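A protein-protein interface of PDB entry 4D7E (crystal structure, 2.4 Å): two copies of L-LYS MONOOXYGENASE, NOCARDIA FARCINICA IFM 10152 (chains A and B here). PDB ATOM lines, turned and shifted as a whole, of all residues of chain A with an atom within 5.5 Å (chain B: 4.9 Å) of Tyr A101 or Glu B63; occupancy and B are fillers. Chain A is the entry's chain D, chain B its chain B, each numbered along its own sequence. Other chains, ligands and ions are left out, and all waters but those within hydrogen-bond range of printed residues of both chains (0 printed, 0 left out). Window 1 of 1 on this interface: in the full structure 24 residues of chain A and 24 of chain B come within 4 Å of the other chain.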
ATOM      1  N   GLU A  63      14.616  -6.375 -25.375  1.00  0.00           N
ATOM      2  CA  GLU A  63      15.406  -5.602 -26.319  1.00  0.00           C
ATOM      3  C   GLU A  63      15.912  -6.542 -27.430  1.00  0.00           C
ATOM      4  O   GLU A  63      16.025  -6.145 -28.569  1.00  0.00           O
ATOM      5  CB  GLU A  63      16.555  -4.881 -25.621  1.00  0.00           C
ATOM      6  CG  GLU A  63      16.094  -3.753 -24.663  1.00  0.00           C
ATOM      7  CD  GLU A  63      15.937  -4.203 -23.219  1.00  0.00           C
ATOM      8  OE1 GLU A  63      15.625  -5.410 -22.979  1.00  0.00           O
ATOM      9  OE2 GLU A  63      16.099  -3.345 -22.311  1.00  0.00           O
ATOM     10  N   THR A  92      11.080  -1.329 -27.676  1.00  0.00           N
ATOM     11  CA  THR A  92      10.898  -0.023 -27.073  1.00  0.00           C
ATOM     12  C   THR A  92       9.928   0.833 -27.917  1.00  0.00           C
ATOM     13  O   THR A  92       9.006   1.478 -27.378  1.00  0.00           O
ATOM     14  CB  THR A  92      12.245   0.706 -26.918  1.00  0.00           C
ATOM     15  OG1 THR A  92      12.976   0.592 -28.128  1.00  0.00           O
ATOM     16  CG2 THR A  92      13.083   0.092 -25.828  1.00  0.00           C
ATOM     17  N   LEU A  95       6.480  -0.332 -27.065  1.00  0.00           N
ATOM     18  CA  LEU A  95       5.954   0.126 -25.790  1.00  0.00           C
ATOM     19  C   LEU A  95       5.486   1.559 -25.888  1.00  0.00           C
ATOM     20  O   LEU A  95       4.466   1.953 -25.310  1.00  0.00           O
ATOM     21  CB  LEU A  95       6.997   0.016 -24.695  1.00  0.00           C
ATOM     22  CG  LEU A  95       7.316  -1.425 -24.324  1.00  0.00           C
ATOM     23  CD1 LEU A  95       8.408  -1.453 -23.283  1.00  0.00           C
ATOM     24  CD2 LEU A  95       6.104  -2.115 -23.775  1.00  0.00           C
ATOM     25  N   VAL A  96       6.240   2.331 -26.655  1.00  0.00           N
ATOM     26  CA  VAL A  96       5.974   3.771 -26.802  1.00  0.00           C
ATOM     27  C   VAL A  96       4.741   4.088 -27.658  1.00  0.00           C
ATOM     28  O   VAL A  96       4.015   4.997 -27.319  1.00  0.00           O
ATOM     29  CB  VAL A  96       7.220   4.457 -27.321  1.00  0.00           C
ATOM     30  CG1 VAL A  96       6.888   5.788 -27.963  1.00  0.00           C
ATOM     31  CG2 VAL A  96       8.235   4.544 -26.197  1.00  0.00           C
ATOM     32  N   GLY A  99       2.142   3.463 -25.258  1.00  0.00           N
ATOM     33  CA  GLY A  99       2.167   4.396 -24.108  1.00  0.00           C
ATOM     34  C   GLY A  99       2.356   3.713 -22.769  1.00  0.00           C
ATOM     35  O   GLY A  99       1.805   4.135 -21.745  1.00  0.00           O
ATOM     36  N   THR A 100       3.137   2.644 -22.795  1.00  0.00           N
ATOM     37  CA  THR A 100       3.368   1.800 -21.627  1.00  0.00           C
ATOM     38  C   THR A 100       4.858   1.692 -21.350  1.00  0.00           C
ATOM     39  O   THR A 100       5.257   0.995 -20.424  1.00  0.00           O
ATOM     40  CB  THR A 100       2.778   0.392 -21.837  1.00  0.00           C
ATOM     41  OG1 THR A 100       3.295  -0.165 -23.045  1.00  0.00           O
ATOM     42  CG2 THR A 100       1.256   0.467 -21.927  1.00  0.00           C
ATOM     43  N   TYR A 101       5.669   2.434 -22.111  1.00  0.00           N
ATOM     44  CA  TYR A 101       7.113   2.469 -21.936  1.00  0.00           C
ATOM     45  C   TYR A 101       7.574   2.917 -20.567  1.00  0.00           C
ATOM     46  O   TYR A 101       8.511   2.328 -20.016  1.00  0.00           O
ATOM     47  CB  TYR A 101       7.716   3.379 -22.978  1.00  0.00           C
ATOM     48  CG  TYR A 101       9.202   3.325 -23.050  1.00  0.00           C
ATOM     49  CD1 TYR A 101       9.893   2.140 -22.835  1.00  0.00           C
ATOM     50  CD2 TYR A 101       9.936   4.463 -23.355  1.00  0.00           C
ATOM     51  CE1 TYR A 101      11.269   2.089 -22.935  1.00  0.00           C
ATOM     52  CE2 TYR A 101      11.317   4.427 -23.448  1.00  0.00           C
ATOM     53  CZ  TYR A 101      11.976   3.235 -23.250  1.00  0.00           C
ATOM     54  OH  TYR A 101      13.338   3.182 -23.353  1.00  0.00           O
ATOM     55  N   ALA A 102       6.887   3.918 -20.003  1.00  0.00           N
ATOM     56  CA  ALA A 102       7.170   4.365 -18.644  1.00  0.00           C
ATOM     57  C   ALA A 102       6.764   3.294 -17.656  1.00  0.00           C
ATOM     58  O   ALA A 102       7.506   2.971 -16.721  1.00  0.00           O
ATOM     59  CB  ALA A 102       6.472   5.685 -18.323  1.00  0.00           C
ATOM     60  N   GLU A 103       5.584   2.742 -17.839  1.00  0.00           N
ATOM     61  CA  GLU A 103       5.198   1.652 -16.961  1.00  0.00           C
ATOM     62  C   GLU A 103       6.286   0.542 -16.968  1.00  0.00           C
ATOM     63  O   GLU A 103       6.707   0.106 -15.913  1.00  0.00           O
ATOM     64  CB  GLU A 103       3.831   1.092 -17.342  1.00  0.00           C
ATOM     65  CG  GLU A 103       3.494  -0.211 -16.661  1.00  0.00           C
ATOM     66  CD  GLU A 103       2.013  -0.414 -16.581  1.00  0.00           C
ATOM     67  OE1 GLU A 103       1.427  -0.945 -17.528  1.00  0.00           O
ATOM     68  OE2 GLU A 103       1.433  -0.028 -15.558  1.00  0.00           O
ATOM     69  N   TRP A 104       6.755   0.143 -18.149  1.00  0.00           N
ATOM     70  CA  TRP A 104       7.810  -0.895 -18.281  1.00  0.00           C
ATOM     71  C   TRP A 104       9.050  -0.530 -17.472  1.00  0.00           C
ATOM     72  O   TRP A 104       9.518  -1.319 -16.635  1.00  0.00           O
ATOM     73  CB  TRP A 104       8.224  -1.126 -19.750  1.00  0.00           C
ATOM     74  CG  TRP A 104       9.159  -2.321 -19.905  1.00  0.00           C
ATOM     75  CD1 TRP A 104       8.899  -3.606 -19.503  1.00  0.00           C
ATOM     76  CD2 TRP A 104      10.487  -2.355 -20.490  1.00  0.00           C
ATOM     77  NE1 TRP A 104       9.969  -4.424 -19.793  1.00  0.00           N
ATOM     78  CE2 TRP A 104      10.947  -3.694 -20.402  1.00  0.00           C
ATOM     79  CE3 TRP A 104      11.305  -1.406 -21.090  1.00  0.00           C
ATOM     80  CZ2 TRP A 104      12.175  -4.098 -20.878  1.00  0.00           C
ATOM     81  CZ3 TRP A 104      12.531  -1.805 -21.558  1.00  0.00           C
ATOM     82  CH2 TRP A 104      12.961  -3.156 -21.446  1.00  0.00           C
ATOM     83  N   ILE A 105       9.552   0.680 -17.710  1.00  0.00           N
ATOM     84  CA  ILE A 105      10.725   1.171 -16.982  1.00  0.00           C
ATOM     85  C   ILE A 105      10.450   1.231 -15.513  1.00  0.00           C
ATOM     86  O   ILE A 105      11.276   0.793 -14.732  1.00  0.00           O
ATOM     87  CB  ILE A 105      11.149   2.583 -17.419  1.00  0.00           C
ATOM     88  CG1 ILE A 105      11.657   2.577 -18.850  1.00  0.00           C
ATOM     89  CG2 ILE A 105      12.227   3.140 -16.495  1.00  0.00           C
ATOM     90  CD1 ILE A 105      12.653   1.506 -19.125  1.00  0.00           C
ATOM     91  N   ASP A 106       9.292   1.763 -15.143  1.00  0.00           N
ATOM     92  CA  ASP A 106       8.971   1.966 -13.744  1.00  0.00           C
ATOM     93  C   ASP A 106       8.739   0.660 -12.996  1.00  0.00           C
ATOM     94  O   ASP A 106       8.902   0.628 -11.772  1.00  0.00           O
ATOM     95  CB  ASP A 106       7.736   2.877 -13.569  1.00  0.00           C
ATOM     96  CG  ASP A 106       8.053   4.375 -13.713  1.00  0.00           C
ATOM     97  OD1 ASP A 106       9.241   4.769 -13.757  1.00  0.00           O
ATOM     98  OD2 ASP A 106       7.082   5.169 -13.755  1.00  0.00           O
ATOM     99  N   ARG A 109      11.561  -3.006 -15.687  1.00  0.00           N
ATOM    100  CA  ARG A 109      11.798  -3.655 -16.979  1.00  0.00           C
ATOM    101  C   ARG A 109      11.417  -5.110 -16.971  1.00  0.00           C
ATOM    102  O   ARG A 109      12.196  -5.937 -17.391  1.00  0.00           O
ATOM    103  CB  ARG A 109      13.258  -3.582 -17.373  1.00  0.00           C
ATOM    104  CG  ARG A 109      13.872  -2.213 -17.345  1.00  0.00           C
ATOM    105  CD  ARG A 109      15.100  -2.282 -18.236  1.00  0.00           C
ATOM    106  NE  ARG A 109      15.977  -1.142 -18.124  1.00  0.00           N
ATOM    107  CZ  ARG A 109      16.958  -0.987 -17.236  1.00  0.00           C
ATOM    108  NH1 ARG A 109      17.205  -1.919 -16.327  1.00  0.00           N
ATOM    109  NH2 ARG A 109      17.709   0.140 -17.262  1.00  0.00           N
ATOM    110  N   SER B  61      17.272   4.716 -14.328  1.00  0.00           N
ATOM    111  CA  SER B  61      17.413   3.962 -15.535  1.00  0.00           C
ATOM    112  C   SER B  61      17.730   4.903 -16.668  1.00  0.00           C
ATOM    113  O   SER B  61      17.002   5.878 -16.879  1.00  0.00           O
ATOM    114  CB  SER B  61      16.108   3.179 -15.838  1.00  0.00           C
ATOM    115  OG  SER B  61      16.010   1.946 -15.109  1.00  0.00           O
ATOM    116  N   PRO B  62      18.777   4.599 -17.452  1.00  0.00           N
ATOM    117  CA  PRO B  62      19.174   5.529 -18.509  1.00  0.00           C
ATOM    118  C   PRO B  62      18.137   5.692 -19.603  1.00  0.00           C
ATOM    119  O   PRO B  62      18.238   6.650 -20.375  1.00  0.00           O
ATOM    120  CB  PRO B  62      20.434   4.893 -19.078  1.00  0.00           C
ATOM    121  CG  PRO B  62      20.254   3.419 -18.747  1.00  0.00           C
ATOM    122  CD  PRO B  62      19.713   3.490 -17.354  1.00  0.00           C
ATOM    123  N   GLU B  63      17.158   4.774 -19.688  1.00  0.00           N
ATOM    124  CA  GLU B  63      16.051   4.950 -20.620  1.00  0.00           C
ATOM    125  C   GLU B  63      15.297   6.253 -20.306  1.00  0.00           C
ATOM    126  O   GLU B  63      14.615   6.767 -21.163  1.00  0.00           O
ATOM    127  CB  GLU B  63      15.043   3.806 -20.561  1.00  0.00           C
ATOM    128  CG  GLU B  63      15.577   2.472 -21.084  1.00  0.00           C
ATOM    129  CD  GLU B  63      16.433   1.775 -20.050  1.00  0.00           C
ATOM    130  OE1 GLU B  63      16.985   2.426 -19.106  1.00  0.00           O
ATOM    131  OE2 GLU B  63      16.554   0.575 -20.148  1.00  0.00           O
ATOM    132  N   LYS B  64      15.346   6.707 -19.048  1.00  0.00           N
ATOM    133  CA  LYS B  64      14.789   8.005 -18.662  1.00  0.00           C
ATOM    134  C   LYS B  64      15.742   9.025 -19.184  1.00  0.00           C
ATOM    135  O   LYS B  64      16.685   9.398 -18.493  1.00  0.00           O
ATOM    136  CB  LYS B  64      14.638   8.129 -17.153  1.00  0.00           C
ATOM    137  CG  LYS B  64      13.836   7.000 -16.570  1.00  0.00           C
ATOM    138  CD  LYS B  64      12.934   7.489 -15.486  1.00  0.00           C
ATOM    139  CE  LYS B  64      11.994   6.407 -15.055  1.00  0.00           C
ATOM    140  NZ  LYS B  64      10.979   7.030 -14.174  1.00  0.00           N
ATOM    141  N   ASP B  65      15.538   9.398 -20.441  1.00  0.00           N
ATOM    142  CA  ASP B  65      16.454  10.281 -21.092  1.00  0.00           C
ATOM    143  C   ASP B  65      15.779  11.572 -21.564  1.00  0.00           C
ATOM    144  O   ASP B  65      14.695  11.951 -21.099  1.00  0.00           O
ATOM    145  CB  ASP B  65      17.070   9.570 -22.263  1.00  0.00           C
ATOM    146  CG  ASP B  65      16.025   9.063 -23.265  1.00  0.00           C
ATOM    147  OD1 ASP B  65      14.855   9.526 -23.210  1.00  0.00           O
ATOM    148  OD2 ASP B  65      16.380   8.146 -24.077  1.00  0.00           O
ATOM    149  N   PHE B  68      12.037  10.944 -22.738  1.00  0.00           N
ATOM    150  CA  PHE B  68      11.201  10.038 -21.988  1.00  0.00           C
ATOM    151  C   PHE B  68      10.026  10.725 -21.307  1.00  0.00           C
ATOM    152  O   PHE B  68      10.196  11.732 -20.598  1.00  0.00           O
ATOM    153  CB  PHE B  68      12.097   9.336 -20.951  1.00  0.00           C
ATOM    154  CG  PHE B  68      11.378   8.426 -20.023  1.00  0.00           C
ATOM    155  CD1 PHE B  68      10.880   8.888 -18.825  1.00  0.00           C
ATOM    156  CD2 PHE B  68      11.260   7.077 -20.326  1.00  0.00           C
ATOM    157  CE1 PHE B  68      10.239   8.023 -17.947  1.00  0.00           C
ATOM    158  CE2 PHE B  68      10.632   6.205 -19.449  1.00  0.00           C
ATOM    159  CZ  PHE B  68      10.114   6.685 -18.261  1.00  0.00           C
ATOM    160  N   PRO B  69       8.838  10.145 -21.428  1.00  0.00           N
ATOM    161  CA  PRO B  69       8.633   8.764 -21.914  1.00  0.00           C
ATOM    162  C   PRO B  69       8.011   8.637 -23.299  1.00  0.00           C
ATOM    163  O   PRO B  69       7.429   7.609 -23.600  1.00  0.00           O
ATOM    164  CB  PRO B  69       7.667   8.206 -20.892  1.00  0.00           C
ATOM    165  CG  PRO B  69       6.784   9.396 -20.600  1.00  0.00           C
ATOM    166  CD  PRO B  69       7.726  10.590 -20.568  1.00  0.00           C
ATOM    167  N   TYR B  70       8.143   9.658 -24.140  1.00  0.00           N
ATOM    168  CA  TYR B  70       7.651   9.614 -25.530  1.00  0.00           C
ATOM    169  C   TYR B  70       6.147   9.343 -25.624  1.00  0.00           C
ATOM    170  O   TYR B  70       5.668   8.506 -26.404  1.00  0.00           O
ATOM    171  CB  TYR B  70       8.458   8.562 -26.305  1.00  0.00           C
ATOM    172  CG  TYR B  70       9.923   8.774 -26.159  1.00  0.00           C
ATOM    173  CD1 TYR B  70      10.577   9.685 -26.945  1.00  0.00           C
ATOM    174  CD2 TYR B  70      10.639   8.107 -25.202  1.00  0.00           C
ATOM    175  CE1 TYR B  70      11.931   9.901 -26.823  1.00  0.00           C
ATOM    176  CE2 TYR B  70      12.001   8.282 -25.077  1.00  0.00           C
ATOM    177  CZ  TYR B  70      12.658   9.180 -25.891  1.00  0.00           C
ATOM    178  OH  TYR B  70      14.030   9.403 -25.745  1.00  0.00           O
ATOM    179  N   TRP B  91      18.735   7.329 -25.345  1.00  0.00           N
ATOM    180  CA  TRP B  91      19.875   6.529 -24.874  1.00  0.00           C
ATOM    181  C   TRP B  91      20.090   5.318 -25.801  1.00  0.00           C
ATOM    182  O   TRP B  91      21.188   5.119 -26.340  1.00  0.00           O
ATOM    183  CB  TRP B  91      19.618   6.125 -23.423  1.00  0.00           C
ATOM    184  CG  TRP B  91      20.474   5.113 -22.893  1.00  0.00           C
ATOM    185  CD1 TRP B  91      20.133   3.800 -22.671  1.00  0.00           C
ATOM    186  CD2 TRP B  91      21.827   5.252 -22.464  1.00  0.00           C
ATOM    187  NE1 TRP B  91      21.184   3.119 -22.144  1.00  0.00           N
ATOM    188  CE2 TRP B  91      22.246   3.975 -22.009  1.00  0.00           C
ATOM    189  CE3 TRP B  91      22.731   6.313 -22.429  1.00  0.00           C
ATOM    190  CZ2 TRP B  91      23.532   3.740 -21.534  1.00  0.00           C
ATOM    191  CZ3 TRP B  91      23.976   6.099 -21.940  1.00  0.00           C
ATOM    192  CH2 TRP B  91      24.384   4.813 -21.512  1.00  0.00           C
ATOM    193  N   TRP B 104      25.692  -3.430 -24.135  1.00  0.00           N
ATOM    194  CA  TRP B 104      24.917  -2.904 -23.034  1.00  0.00           C
ATOM    195  C   TRP B 104      23.917  -3.965 -22.579  1.00  0.00           C
ATOM    196  O   TRP B 104      23.919  -4.364 -21.407  1.00  0.00           O
ATOM    197  CB  TRP B 104      24.229  -1.564 -23.390  1.00  0.00           C
ATOM    198  CG  TRP B 104      23.580  -0.965 -22.184  1.00  0.00           C
ATOM    199  CD1 TRP B 104      24.196  -0.592 -21.011  1.00  0.00           C
ATOM    200  CD2 TRP B 104      22.196  -0.706 -22.000  1.00  0.00           C
ATOM    201  NE1 TRP B 104      23.271  -0.159 -20.111  1.00  0.00           N
ATOM    202  CE2 TRP B 104      22.038  -0.182 -20.703  1.00  0.00           C
ATOM    203  CE3 TRP B 104      21.066  -0.888 -22.796  1.00  0.00           C
ATOM    204  CZ2 TRP B 104      20.810   0.139 -20.185  1.00  0.00           C
ATOM    205  CZ3 TRP B 104      19.848  -0.532 -22.283  1.00  0.00           C
ATOM    206  CH2 TRP B 104      19.731  -0.030 -20.983  1.00  0.00           C
ATOM    207  N   ARG B 109      22.458  -4.392 -18.844  1.00  0.00           N
ATOM    208  CA  ARG B 109      22.034  -3.010 -18.809  1.00  0.00           C
ATOM    209  C   ARG B 109      22.719  -2.296 -17.628  1.00  0.00           C
ATOM    210  O   ARG B 109      22.065  -1.755 -16.755  1.00  0.00           O
ATOM    211  CB  ARG B 109      20.513  -2.924 -18.674  1.00  0.00           C
ATOM    212  CG  ARG B 109      19.700  -3.776 -19.646  1.00  0.00           C
ATOM    213  CD  ARG B 109      18.250  -3.336 -19.544  1.00  0.00           C
ATOM    214  NE  ARG B 109      17.279  -4.231 -20.154  1.00  0.00           N
ATOM    215  CZ  ARG B 109      16.629  -5.195 -19.514  1.00  0.00           C
ATOM    216  NH1 ARG B 109      16.861  -5.457 -18.244  1.00  0.00           N
ATOM    217  NH2 ARG B 109      15.740  -5.923 -20.163  1.00  0.00           N
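Printed residues of chain B within 4 Å of Asp A106: Lys B64.
Printed residues of chain A within 4 Å of Lys B64: Ile A105 (3.6 Å) and Asp A106 (2.9 Å).
Printed residues of chain A within 4 Å of Tyr B70: Val A96.
The nearest residue of chain B that does not touch Tyr A101 is Pro B69 (4.03 Å).
OD1 of Asp B65 lies within hydrogen-bond range of N of Phe B68, 3.2 Å away.
The side-chain hydroxyl of Tyr B70 lies within hydrogen-bond range of the side-chain carboxylate of Asp B65 (2.7 Å).
The backbone carbonyl oxygen of Trp B104 lies within hydrogen-bond range of the backbone NH of Arg B109, at 3.0 Å.
O of Leu A95 sits at hydrogen-bond distance from N of Tyr A101 (3.5 Å).
The backbone carbonyl oxygen (O) of Trp A104 lies within hydrogen-bond range of the backbone NH (N) of Arg A109 (2.8 Å).
Tyr B70 touches Val A96.
CG of Glu B63 touches OH of Tyr A101, at 3.3 Å.
Ala A102 touches Phe B68.
Ala A102 touches Pro B69.
Ser B61 touches Ile A105 (CB to CG2, 3.9 Å).
Ile A105 touches Glu B63.
Lys B64 touches Ile A105 (CE to CG2, 3.6 Å).
Ile A105 touches Phe B68 (CG1 to CE2, 3.8 Å).
CD of Pro B62 touches NH2 of Arg A109, at 3.9 Å.
CD of Arg B109 touches NE of Arg A109, at 3.5 Å.
Printed residues of chain B that touch a printed residue of chain A: Ser B61, Pro B62, Glu B63, Lys B64, Phe B68, Pro B69, Tyr B70 and Arg B109.
Hydrophobic or aromatic side chains of chain B within 4 Å of the printed part of chain A: Pro B62, Phe B68, Pro B69 and Tyr B70.
Printed residues of chain A that touch a printed residue of chain B: Glu A63, Val A96, Tyr A101, Ala A102, Ile A105, Asp A106 and Arg A109.
Among the printed residues, 14 pairs touch across the chains.
Among the printed residues, Asp or Glu carboxylates within 4 Å of a Lys or Arg side-chain nitrogen of the other chain: Glu A63 with Arg B109 (2.6 Å), Asp A106 with Lys B64 (2.9 Å) and Arg A109 with Glu B63 (2.7 Å).
Glu A63 touches Arg B109, and with the chains exchanged Arg A109 touches Glu B63.
Arg A109 touches its own counterpart, Arg B109.
3 positions are printed for both chains.
Of the 14 pairs that touch across the chains among the printed residues, 3 have their exchanged pair printed and touching as well.
NH2 of Arg A109 is in hydrogen-bond range of OG of Ser B61, 3.3 Å away.
OE2 of Glu B63 is in salt-bridge range of NE of Arg A109, 2.7 Å away.
OD1 of Asp A106 lies within salt-bridge range of NZ of Lys B64 (2.9 Å).
NE of Arg B109 lies within salt-bridge range of OE2 of Glu A63 (2.6 Å).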
